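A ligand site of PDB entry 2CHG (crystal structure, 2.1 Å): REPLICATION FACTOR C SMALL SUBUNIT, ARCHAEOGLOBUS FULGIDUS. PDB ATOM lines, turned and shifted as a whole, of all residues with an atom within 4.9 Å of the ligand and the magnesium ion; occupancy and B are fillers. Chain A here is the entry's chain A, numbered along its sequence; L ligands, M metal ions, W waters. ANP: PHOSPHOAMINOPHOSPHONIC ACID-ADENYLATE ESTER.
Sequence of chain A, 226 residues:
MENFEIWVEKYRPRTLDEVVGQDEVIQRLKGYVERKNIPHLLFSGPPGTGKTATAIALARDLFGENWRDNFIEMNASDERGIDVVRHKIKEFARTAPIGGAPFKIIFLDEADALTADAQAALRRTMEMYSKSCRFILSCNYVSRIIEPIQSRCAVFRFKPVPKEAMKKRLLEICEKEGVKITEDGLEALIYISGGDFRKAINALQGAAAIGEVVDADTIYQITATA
The backbone NH of Lys 51 lies within hydrogen-bond range of an oxygen (O3G) of the ligand (2.7 Å). An oxygen (O2G) of the ligand sits at hydrogen-bond distance from the backbone NH (N) of Thr 52 (3.0 Å). N of Thr 49 lies within hydrogen-bond range of O3G of the ligand. N6 of the ligand is in hydrogen-bond range of O of Thr 49, at 3.0 Å. O of Val 8 lies within hydrogen-bond range of O3' of the ligand, 2.6 Å away. N of Gly 48 sits close to O1G of the ligand. The backbone carbonyl oxygen (O) of Tyr 11 lies within hydrogen-bond range of an oxygen (O2') of the ligand. The backbone NH (N) of Ala 53 lies within hydrogen-bond range of an oxygen (O2A) of the ligand (2.8 Å). N of Val 20 lies within hydrogen-bond range of N1 of the ligand (3.0 Å). NH1 of Arg 12 lies within salt-bridge range of O1A of the ligand. An oxygen (O2G) of the ligand is in hydrogen-bond range of the side-chain hydroxyl of Thr 52 (2.6 Å). O1B of the ligand lies within salt-bridge range of NH1 of Arg 198 (3.7 Å). The backbone NH (N) of Gly 50 sits at hydrogen-bond distance from an oxygen (O3G) of the ligand, 3.1 Å away. An oxygen (O3G) of the ligand lies within salt-bridge range of the side-chain amino group (NZ) of Lys 51 (2.7 Å). A nitrogen (N6) of the ligand sits at hydrogen-bond distance from the backbone carbonyl oxygen (O) of Val 20, at 2.9 Å.
The guanidinium group of Arg 12 lies within salt-bridge range of the side-chain carboxylate of Glu 9. NH1 of Arg 169 lies close to O of Glu 18 (3.5 Å). The side-chain amide nitrogen of Gln 22 sits at hydrogen-bond distance from the backbone carbonyl oxygen of Thr 49. The backbone NH (N) of Arg 198 sits close to the side-chain carboxylate (OD1) of Asp 196. The side-chain amino group (NZ) of Lys 51 lies within hydrogen-bond range of the backbone carbonyl oxygen (O) of Pro 46. The backbone carbonyl oxygen (O) of Pro 46 sits at hydrogen-bond distance from the side-chain hydroxyl (OG1) of Thr 49 (2.8 Å).
Merely in contact with the ligand: Pro 13 (3.2 Å), Phe 197 (3.3 Å), Ile 201 (3.7 Å), Pro 47 (3.7 Å), Arg 169 (3.8 Å), Val 19 (3.8 Å) and Glu 18 (3.9 Å). Of the 24 residues printed, 18 come within 4 Å of the ligand. The nearest printed residue that does not touch the ligand is Pro 46 (4.2 Å).
Residues that only touch the magnesium ion: Gly 48. Of the 24 residues printed, 1 comes within 4 Å of the magnesium ion. The nearest printed residue that does not touch the magnesium ion is Pro 47 (4.7 Å).
The magnesium ion is bound by water W1 (1.9 Å), water W4 (1.9 Å), O1G of the ligand (1.9 Å), water W2 (2.0 Å), water W3 (2.1 Å) and O2B of the ligand (2.1 Å). The magnesium ion has six donor atoms within binding distance.
Water W9 lies within hydrogen-bond range of an oxygen (O1A) of the ligand (2.7 Å), the guanidinium group of Arg 198 (3.1 Å) and the guanidinium group of Arg 12 (3.4 Å). Water W7 bridges O2G of the ligand (2.7 Å) and OG1 of Thr 52 (3.4 Å). Water W5 lies within hydrogen-bond range of O of Gly 48 (2.7 Å), O1B of the ligand (2.8 Å), N of Phe 197 (3.1 Å) and N of Arg 198 (3.5 Å). Water W8 lies within hydrogen-bond range of the side-chain carboxylate of Asp 196 (2.7 Å) and an oxygen (O1B) of the ligand (2.8 Å). Water W6 lies within hydrogen-bond range of O of Tyr 11, O2' of the ligand and NE of Arg 169.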
ATOM      1  N   TRP A   7     -13.058 -10.770   1.763  1.00  0.00           N
ATOM      2  CA  TRP A   7     -13.249 -10.124   3.043  1.00  0.00           C
ATOM      3  C   TRP A   7     -14.658 -10.403   3.563  1.00  0.00           C
ATOM      4  O   TRP A   7     -14.884 -10.418   4.756  1.00  0.00           O
ATOM      5  CB  TRP A   7     -12.950  -8.627   2.962  1.00  0.00           C
ATOM      6  CG  TRP A   7     -11.465  -8.283   2.793  1.00  0.00           C
ATOM      7  CD1 TRP A   7     -10.428  -9.155   2.605  1.00  0.00           C
ATOM      8  CD2 TRP A   7     -10.882  -6.972   2.771  1.00  0.00           C
ATOM      9  NE1 TRP A   7      -9.234  -8.468   2.500  1.00  0.00           N
ATOM     10  CE2 TRP A   7      -9.486  -7.132   2.590  1.00  0.00           C
ATOM     11  CE3 TRP A   7     -11.411  -5.674   2.891  1.00  0.00           C
ATOM     12  CZ2 TRP A   7      -8.611  -6.033   2.511  1.00  0.00           C
ATOM     13  CZ3 TRP A   7     -10.529  -4.585   2.831  1.00  0.00           C
ATOM     14  CH2 TRP A   7      -9.149  -4.792   2.636  1.00  0.00           C
ATOM     15  N   VAL A   8     -15.578 -10.677   2.633  1.00  0.00           N
ATOM     16  CA  VAL A   8     -16.949 -11.070   2.973  1.00  0.00           C
ATOM     17  C   VAL A   8     -16.905 -12.304   3.896  1.00  0.00           C
ATOM     18  O   VAL A   8     -17.718 -12.427   4.807  1.00  0.00           O
ATOM     19  CB  VAL A   8     -17.815 -11.271   1.701  1.00  0.00           C
ATOM     20  CG1 VAL A   8     -18.961 -12.290   1.891  1.00  0.00           C
ATOM     21  CG2 VAL A   8     -18.360  -9.939   1.211  1.00  0.00           C
ATOM     22  N   GLU A   9     -15.905 -13.165   3.675  1.00  0.00           N
ATOM     23  CA  GLU A   9     -15.734 -14.368   4.503  1.00  0.00           C
ATOM     24  C   GLU A   9     -14.748 -14.195   5.643  1.00  0.00           C
ATOM     25  O   GLU A   9     -15.023 -14.581   6.785  1.00  0.00           O
ATOM     26  CB  GLU A   9     -15.347 -15.575   3.635  1.00  0.00           C
ATOM     27  CG  GLU A   9     -16.470 -16.064   2.746  1.00  0.00           C
ATOM     28  CD  GLU A   9     -17.669 -16.562   3.544  1.00  0.00           C
ATOM     29  OE1 GLU A   9     -18.793 -16.478   3.013  1.00  0.00           O
ATOM     30  OE2 GLU A   9     -17.486 -17.009   4.692  1.00  0.00           O
ATOM     31  N   TYR A  11     -14.261 -11.587   7.217  1.00  0.00           N
ATOM     32  CA  TYR A  11     -14.889 -10.768   8.270  1.00  0.00           C
ATOM     33  C   TYR A  11     -16.368 -11.128   8.540  1.00  0.00           C
ATOM     34  O   TYR A  11     -17.172 -10.305   8.946  1.00  0.00           O
ATOM     35  CB  TYR A  11     -14.644  -9.272   7.977  1.00  0.00           C
ATOM     36  CG  TYR A  11     -13.162  -8.966   8.010  1.00  0.00           C
ATOM     37  CD1 TYR A  11     -12.433  -8.779   6.833  1.00  0.00           C
ATOM     38  CD2 TYR A  11     -12.463  -8.961   9.221  1.00  0.00           C
ATOM     39  CE1 TYR A  11     -11.054  -8.536   6.875  1.00  0.00           C
ATOM     40  CE2 TYR A  11     -11.092  -8.729   9.266  1.00  0.00           C
ATOM     41  CZ  TYR A  11     -10.395  -8.515   8.094  1.00  0.00           C
ATOM     42  OH  TYR A  11      -9.047  -8.292   8.143  1.00  0.00           O
ATOM     43  N   ARG A  12     -16.678 -12.398   8.314  1.00  0.00           N
ATOM     44  CA  ARG A  12     -17.969 -12.999   8.633  1.00  0.00           C
ATOM     45  C   ARG A  12     -18.027 -13.260  10.154  1.00  0.00           C
ATOM     46  O   ARG A  12     -17.048 -13.732  10.736  1.00  0.00           O
ATOM     47  CB  ARG A  12     -18.074 -14.311   7.837  1.00  0.00           C
ATOM     48  CG  ARG A  12     -18.990 -15.356   8.435  1.00  0.00           C
ATOM     49  CD  ARG A  12     -19.176 -16.587   7.553  1.00  0.00           C
ATOM     50  NE  ARG A  12     -19.603 -16.288   6.179  1.00  0.00           N
ATOM     51  CZ  ARG A  12     -20.756 -15.714   5.811  1.00  0.00           C
ATOM     52  NH1 ARG A  12     -21.664 -15.308   6.716  1.00  0.00           N
ATOM     53  NH2 ARG A  12     -20.987 -15.501   4.536  1.00  0.00           N
ATOM     54  N   PRO A  13     -19.170 -12.934  10.803  1.00  0.00           N
ATOM     55  CA  PRO A  13     -19.312 -13.269  12.235  1.00  0.00           C
ATOM     56  C   PRO A  13     -18.945 -14.732  12.554  1.00  0.00           C
ATOM     57  O   PRO A  13     -19.415 -15.645  11.880  1.00  0.00           O
ATOM     58  CB  PRO A  13     -20.798 -13.036  12.490  1.00  0.00           C
ATOM     59  CG  PRO A  13     -21.165 -11.957  11.534  1.00  0.00           C
ATOM     60  CD  PRO A  13     -20.359 -12.238  10.290  1.00  0.00           C
ATOM     61  N   GLU A  18     -20.983 -11.307  17.246  1.00  0.00           N
ATOM     62  CA  GLU A  18     -20.378 -10.587  16.135  1.00  0.00           C
ATOM     63  C   GLU A  18     -21.389 -10.193  15.070  1.00  0.00           C
ATOM     64  O   GLU A  18     -21.060  -9.418  14.175  1.00  0.00           O
ATOM     65  CB  GLU A  18     -19.212 -11.386  15.550  1.00  0.00           C
ATOM     66  CG  GLU A  18     -17.981 -11.254  16.434  1.00  0.00           C
ATOM     67  CD  GLU A  18     -16.797 -12.053  15.982  1.00  0.00           C
ATOM     68  OE1 GLU A  18     -15.802 -12.024  16.732  1.00  0.00           O
ATOM     69  OE2 GLU A  18     -16.811 -12.702  14.913  1.00  0.00           O
ATOM     70  N   VAL A  19     -22.609 -10.718  15.150  1.00  0.00           N
ATOM     71  CA  VAL A  19     -23.655 -10.159  14.296  1.00  0.00           C
ATOM     72  C   VAL A  19     -24.217  -8.839  14.835  1.00  0.00           C
ATOM     73  O   VAL A  19     -24.421  -8.637  16.037  1.00  0.00           O
ATOM     74  CB  VAL A  19     -24.705 -11.190  13.688  1.00  0.00           C
ATOM     75  CG1 VAL A  19     -24.441 -12.626  14.115  1.00  0.00           C
ATOM     76  CG2 VAL A  19     -26.154 -10.728  13.872  1.00  0.00           C
ATOM     77  N   VAL A  20     -24.452  -7.935  13.905  1.00  0.00           N
ATOM     78  CA  VAL A  20     -24.719  -6.553  14.235  1.00  0.00           C
ATOM     79  C   VAL A  20     -26.144  -6.170  13.818  1.00  0.00           C
ATOM     80  O   VAL A  20     -26.706  -6.761  12.883  1.00  0.00           O
ATOM     81  CB  VAL A  20     -23.583  -5.678  13.594  1.00  0.00           C
ATOM     82  CG1 VAL A  20     -24.079  -4.738  12.487  1.00  0.00           C
ATOM     83  CG2 VAL A  20     -22.787  -5.032  14.647  1.00  0.00           C
ATOM     84  N   GLN A  22     -29.063  -6.692  15.228  1.00  0.00           N
ATOM     85  CA  GLN A  22     -30.147  -7.669  15.492  1.00  0.00           C
ATOM     86  C   GLN A  22     -30.174  -8.148  16.940  1.00  0.00           C
ATOM     87  O   GLN A  22     -30.443  -9.335  17.207  1.00  0.00           O
ATOM     88  CB  GLN A  22     -30.042  -8.904  14.566  1.00  0.00           C
ATOM     89  CG  GLN A  22     -29.723  -8.643  13.075  1.00  0.00           C
ATOM     90  CD  GLN A  22     -30.855  -7.954  12.315  1.00  0.00           C
ATOM     91  OE1 GLN A  22     -32.021  -7.937  12.771  1.00  0.00           O
ATOM     92  NE2 GLN A  22     -30.519  -7.362  11.161  1.00  0.00           N
ATOM     93  N   PRO A  46     -35.657  -8.716   5.638  1.00  0.00           N
ATOM     94  CA  PRO A  46     -35.178  -8.229   4.339  1.00  0.00           C
ATOM     95  C   PRO A  46     -33.854  -8.886   3.906  1.00  0.00           C
ATOM     96  O   PRO A  46     -33.071  -9.329   4.747  1.00  0.00           O
ATOM     97  CB  PRO A  46     -34.973  -6.716   4.572  1.00  0.00           C
ATOM     98  CG  PRO A  46     -35.908  -6.391   5.728  1.00  0.00           C
ATOM     99  CD  PRO A  46     -35.901  -7.601   6.593  1.00  0.00           C
ATOM    100  N   PRO A  47     -33.609  -8.948   2.583  1.00  0.00           N
ATOM    101  CA  PRO A  47     -32.379  -9.547   2.116  1.00  0.00           C
ATOM    102  C   PRO A  47     -31.172  -8.807   2.654  1.00  0.00           C
ATOM    103  O   PRO A  47     -31.210  -7.601   2.806  1.00  0.00           O
ATOM    104  CB  PRO A  47     -32.459  -9.414   0.566  1.00  0.00           C
ATOM    105  CG  PRO A  47     -33.627  -8.608   0.262  1.00  0.00           C
ATOM    106  CD  PRO A  47     -34.489  -8.490   1.492  1.00  0.00           C
ATOM    107  N   GLY A  48     -30.107  -9.539   2.964  1.00  0.00           N
ATOM    108  CA  GLY A  48     -28.848  -8.934   3.360  1.00  0.00           C
ATOM    109  C   GLY A  48     -28.810  -8.409   4.776  1.00  0.00           C
ATOM    110  O   GLY A  48     -27.884  -7.699   5.115  1.00  0.00           O
ATOM    111  N   THR A  49     -29.817  -8.718   5.616  1.00  0.00           N
ATOM    112  CA  THR A  49     -29.798  -8.258   7.009  1.00  0.00           C
ATOM    113  C   THR A  49     -28.975  -9.138   7.970  1.00  0.00           C
ATOM    114  O   THR A  49     -28.742  -8.750   9.140  1.00  0.00           O
ATOM    115  CB  THR A  49     -31.210  -8.088   7.579  1.00  0.00           C
ATOM    116  OG1 THR A  49     -31.960  -9.275   7.340  1.00  0.00           O
ATOM    117  CG2 THR A  49     -31.900  -6.901   6.935  1.00  0.00           C
ATOM    118  N   GLY A  50     -28.539 -10.294   7.495  1.00  0.00           N
ATOM    119  CA  GLY A  50     -27.664 -11.174   8.221  1.00  0.00           C
ATOM    120  C   GLY A  50     -28.259 -12.503   8.642  1.00  0.00           C
ATOM    121  O   GLY A  50     -27.830 -13.084   9.639  1.00  0.00           O
ATOM    122  N   LYS A  51     -29.268 -12.988   7.910  1.00  0.00           N
ATOM    123  CA  LYS A  51     -29.950 -14.218   8.301  1.00  0.00           C
ATOM    124  C   LYS A  51     -28.978 -15.419   8.145  1.00  0.00           C
ATOM    125  O   LYS A  51     -28.816 -16.232   9.056  1.00  0.00           O
ATOM    126  CB  LYS A  51     -31.247 -14.397   7.497  1.00  0.00           C
ATOM    127  CG  LYS A  51     -32.250 -13.258   7.749  1.00  0.00           C
ATOM    128  CD  LYS A  51     -33.577 -13.344   6.998  1.00  0.00           C
ATOM    129  CE  LYS A  51     -33.431 -13.254   5.489  1.00  0.00           C
ATOM    130  NZ  LYS A  51     -32.680 -12.066   4.968  1.00  0.00           N
ATOM    131  N   THR A  52     -28.327 -15.506   6.986  1.00  0.00           N
ATOM    132  CA  THR A  52     -27.352 -16.555   6.746  1.00  0.00           C
ATOM    133  C   THR A  52     -26.224 -16.405   7.732  1.00  0.00           C
ATOM    134  O   THR A  52     -25.832 -17.376   8.356  1.00  0.00           O
ATOM    135  CB  THR A  52     -26.820 -16.517   5.303  1.00  0.00           C
ATOM    136  OG1 THR A  52     -27.916 -16.500   4.379  1.00  0.00           O
ATOM    137  CG2 THR A  52     -25.941 -17.746   5.032  1.00  0.00           C
ATOM    138  N   ALA A  53     -25.693 -15.198   7.903  1.00  0.00           N
ATOM    139  CA  ALA A  53     -24.593 -14.987   8.865  1.00  0.00           C
ATOM    140  C   ALA A  53     -24.922 -15.451  10.291  1.00  0.00           C
ATOM    141  O   ALA A  53     -24.065 -16.035  10.993  1.00  0.00           O
ATOM    142  CB  ALA A  53     -24.168 -13.525   8.900  1.00  0.00           C
ATOM    143  N   VAL A 161     -30.442  -3.137   8.958  1.00  0.00           N
ATOM    144  CA  VAL A 161     -29.338  -2.649   9.786  1.00  0.00           C
ATOM    145  C   VAL A 161     -29.086  -1.154   9.587  1.00  0.00           C
ATOM    146  O   VAL A 161     -28.949  -0.685   8.446  1.00  0.00           O
ATOM    147  CB  VAL A 161     -28.039  -3.553   9.791  1.00  0.00           C
ATOM    148  CG1 VAL A 161     -28.193  -4.802   8.979  1.00  0.00           C
ATOM    149  CG2 VAL A 161     -26.784  -2.782   9.484  1.00  0.00           C
ATOM    150  N   ARG A 169     -18.886  -1.185  11.812  1.00  0.00           N
ATOM    151  CA  ARG A 169     -18.315  -2.445  11.357  1.00  0.00           C
ATOM    152  C   ARG A 169     -17.323  -2.294  10.216  1.00  0.00           C
ATOM    153  O   ARG A 169     -16.298  -2.962  10.172  1.00  0.00           O
ATOM    154  CB  ARG A 169     -19.428  -3.373  10.916  1.00  0.00           C
ATOM    155  CG  ARG A 169     -18.946  -4.734  10.617  1.00  0.00           C
ATOM    156  CD  ARG A 169     -18.131  -5.292  11.802  1.00  0.00           C
ATOM    157  NE  ARG A 169     -18.596  -6.649  11.943  1.00  0.00           N
ATOM    158  CZ  ARG A 169     -19.068  -7.204  13.029  1.00  0.00           C
ATOM    159  NH1 ARG A 169     -19.077  -6.582  14.210  1.00  0.00           N
ATOM    160  NH2 ARG A 169     -19.480  -8.449  12.909  1.00  0.00           N
ATOM    161  N   ASP A 196     -26.693  -3.120   2.406  1.00  0.00           N
ATOM    162  CA  ASP A 196     -26.198  -4.483   2.177  1.00  0.00           C
ATOM    163  C   ASP A 196     -24.688  -4.651   2.508  1.00  0.00           C
ATOM    164  O   ASP A 196     -23.822  -4.148   1.770  1.00  0.00           O
ATOM    165  CB  ASP A 196     -26.466  -4.851   0.719  1.00  0.00           C
ATOM    166  CG  ASP A 196     -26.206  -6.299   0.435  1.00  0.00           C
ATOM    167  OD1 ASP A 196     -25.083  -6.657   0.029  1.00  0.00           O
ATOM    168  OD2 ASP A 196     -27.147  -7.106   0.614  1.00  0.00           O
ATOM    169  N   PHE A 197     -24.390  -5.406   3.572  1.00  0.00           N
ATOM    170  CA  PHE A 197     -23.014  -5.595   4.051  1.00  0.00           C
ATOM    171  C   PHE A 197     -22.134  -6.274   3.001  1.00  0.00           C
ATOM    172  O   PHE A 197     -20.984  -5.931   2.858  1.00  0.00           O
ATOM    173  CB  PHE A 197     -22.961  -6.429   5.337  1.00  0.00           C
ATOM    174  CG  PHE A 197     -22.889  -5.630   6.633  1.00  0.00           C
ATOM    175  CD1 PHE A 197     -23.909  -5.717   7.579  1.00  0.00           C
ATOM    176  CD2 PHE A 197     -21.775  -4.855   6.947  1.00  0.00           C
ATOM    177  CE1 PHE A 197     -23.853  -5.031   8.813  1.00  0.00           C
ATOM    178  CE2 PHE A 197     -21.699  -4.164   8.160  1.00  0.00           C
ATOM    179  CZ  PHE A 197     -22.748  -4.255   9.104  1.00  0.00           C
ATOM    180  N   ARG A 198     -22.675  -7.253   2.281  1.00  0.00           N
ATOM    181  CA  ARG A 198     -21.921  -7.985   1.276  1.00  0.00           C
ATOM    182  C   ARG A 198     -21.419  -7.052   0.166  1.00  0.00           C
ATOM    183  O   ARG A 198     -20.244  -7.108  -0.191  1.00  0.00           O
ATOM    184  CB  ARG A 198     -22.752  -9.145   0.707  1.00  0.00           C
ATOM    185  CG  ARG A 198     -22.307  -9.710  -0.615  1.00  0.00           C
ATOM    186  CD  ARG A 198     -23.077 -11.029  -0.924  1.00  0.00           C
ATOM    187  NE  ARG A 198     -22.407 -12.181  -0.318  1.00  0.00           N
ATOM    188  CZ  ARG A 198     -22.994 -13.126   0.403  1.00  0.00           C
ATOM    189  NH1 ARG A 198     -24.320 -13.120   0.596  1.00  0.00           N
ATOM    190  NH2 ARG A 198     -22.242 -14.127   0.916  1.00  0.00           N
ATOM    191  N   ILE A 201     -18.730  -4.525   1.763  1.00  0.00           N
ATOM    192  CA  ILE A 201     -17.426  -5.143   2.039  1.00  0.00           C
ATOM    193  C   ILE A 201     -16.704  -5.516   0.743  1.00  0.00           C
ATOM    194  O   ILE A 201     -15.471  -5.394   0.651  1.00  0.00           O
ATOM    195  CB  ILE A 201     -17.535  -6.365   3.001  1.00  0.00           C
ATOM    196  CG1 ILE A 201     -18.021  -5.909   4.380  1.00  0.00           C
ATOM    197  CG2 ILE A 201     -16.178  -7.076   3.145  1.00  0.00           C
ATOM    198  CD1 ILE A 201     -18.549  -7.018   5.258  1.00  0.00           C
HETATM  199  PG  ANP L   1     -29.220 -12.706   4.261  1.00  0.00           P
HETATM  200  O1G ANP L   1     -29.770 -12.253   2.922  1.00  0.00           O
HETATM  201  O2G ANP L   1     -29.101 -14.203   4.354  1.00  0.00           O
HETATM  202  O3G ANP L   1     -29.982 -12.103   5.423  1.00  0.00           O
HETATM  203  PB  ANP L   1     -26.602 -12.257   3.178  1.00  0.00           P
HETATM  204  O1B ANP L   1     -25.975 -10.907   3.009  1.00  0.00           O
HETATM  205  O2B ANP L   1     -27.149 -12.909   1.940  1.00  0.00           O
HETATM  206  N3B ANP L   1     -27.722 -12.149   4.350  1.00  0.00           N
HETATM  207  PA  ANP L   1     -24.612 -13.241   5.052  1.00  0.00           P
HETATM  208  O1A ANP L   1     -23.711 -14.470   5.032  1.00  0.00           O
HETATM  209  O2A ANP L   1     -25.637 -13.036   6.144  1.00  0.00           O
HETATM  210  O3A ANP L   1     -25.436 -13.297   3.645  1.00  0.00           O
HETATM  211  O5' ANP L   1     -23.709 -11.917   4.963  1.00  0.00           O
HETATM  212  C5' ANP L   1     -22.657 -11.842   4.004  1.00  0.00           C
HETATM  213  C4' ANP L   1     -21.608 -10.812   4.423  1.00  0.00           C
HETATM  214  O4' ANP L   1     -22.152  -9.632   5.012  1.00  0.00           O
HETATM  215  C3' ANP L   1     -20.657 -11.346   5.478  1.00  0.00           C
HETATM  216  O3' ANP L   1     -19.439 -10.616   5.322  1.00  0.00           O
HETATM  217  C2' ANP L   1     -21.155 -10.849   6.799  1.00  0.00           C
HETATM  218  O2' ANP L   1     -20.043 -10.475   7.603  1.00  0.00           O
HETATM  219  C1' ANP L   1     -21.829  -9.563   6.413  1.00  0.00           C
HETATM  220  N9  ANP L   1     -23.057  -9.345   7.208  1.00  0.00           N
HETATM  221  C8  ANP L   1     -24.321  -9.456   6.742  1.00  0.00           C
HETATM  222  N7  ANP L   1     -25.201  -9.177   7.712  1.00  0.00           N
HETATM  223  C5  ANP L   1     -24.513  -8.874   8.822  1.00  0.00           C
HETATM  224  C6  ANP L   1     -24.853  -8.491  10.197  1.00  0.00           C
HETATM  225  N6  ANP L   1     -26.152  -8.367  10.579  1.00  0.00           N
HETATM  226  N1  ANP L   1     -23.836  -8.275  11.020  1.00  0.00           N
HETATM  227  C2  ANP L   1     -22.532  -8.385  10.676  1.00  0.00           C
HETATM  228  N3  ANP L   1     -22.152  -8.734   9.450  1.00  0.00           N
HETATM  229  C4  ANP L   1     -23.086  -8.994   8.495  1.00  0.00           C
HETATM  230 MG    MG M   1     -29.124 -12.812   1.171  1.00  0.00          MG
HETATM  231  O   HOH W   1     -30.862 -12.954   0.428  1.00  0.00           O
HETATM  232  O   HOH W   2     -28.751 -11.051   0.362  1.00  0.00           O
HETATM  233  O   HOH W   3     -28.271 -13.681  -0.533  1.00  0.00           O
HETATM  234  O   HOH W   4     -29.207 -14.678   1.607  1.00  0.00           O
HETATM  235  O   HOH W   5     -25.710  -8.208   3.658  1.00  0.00           O
HETATM  236  O   HOH W   6     -19.117  -8.567   9.592  1.00  0.00           O
HETATM  237  O   HOH W   7     -31.252 -15.835   3.938  1.00  0.00           O
HETATM  238  O   HOH W   8     -26.477  -9.764   0.503  1.00  0.00           O
HETATM  239  O   HOH W   9     -23.843 -15.983   2.777  1.00  0.00           O
HETATM  240  O   HOH W  10     -33.018 -12.831   2.241  1.00  0.00           O
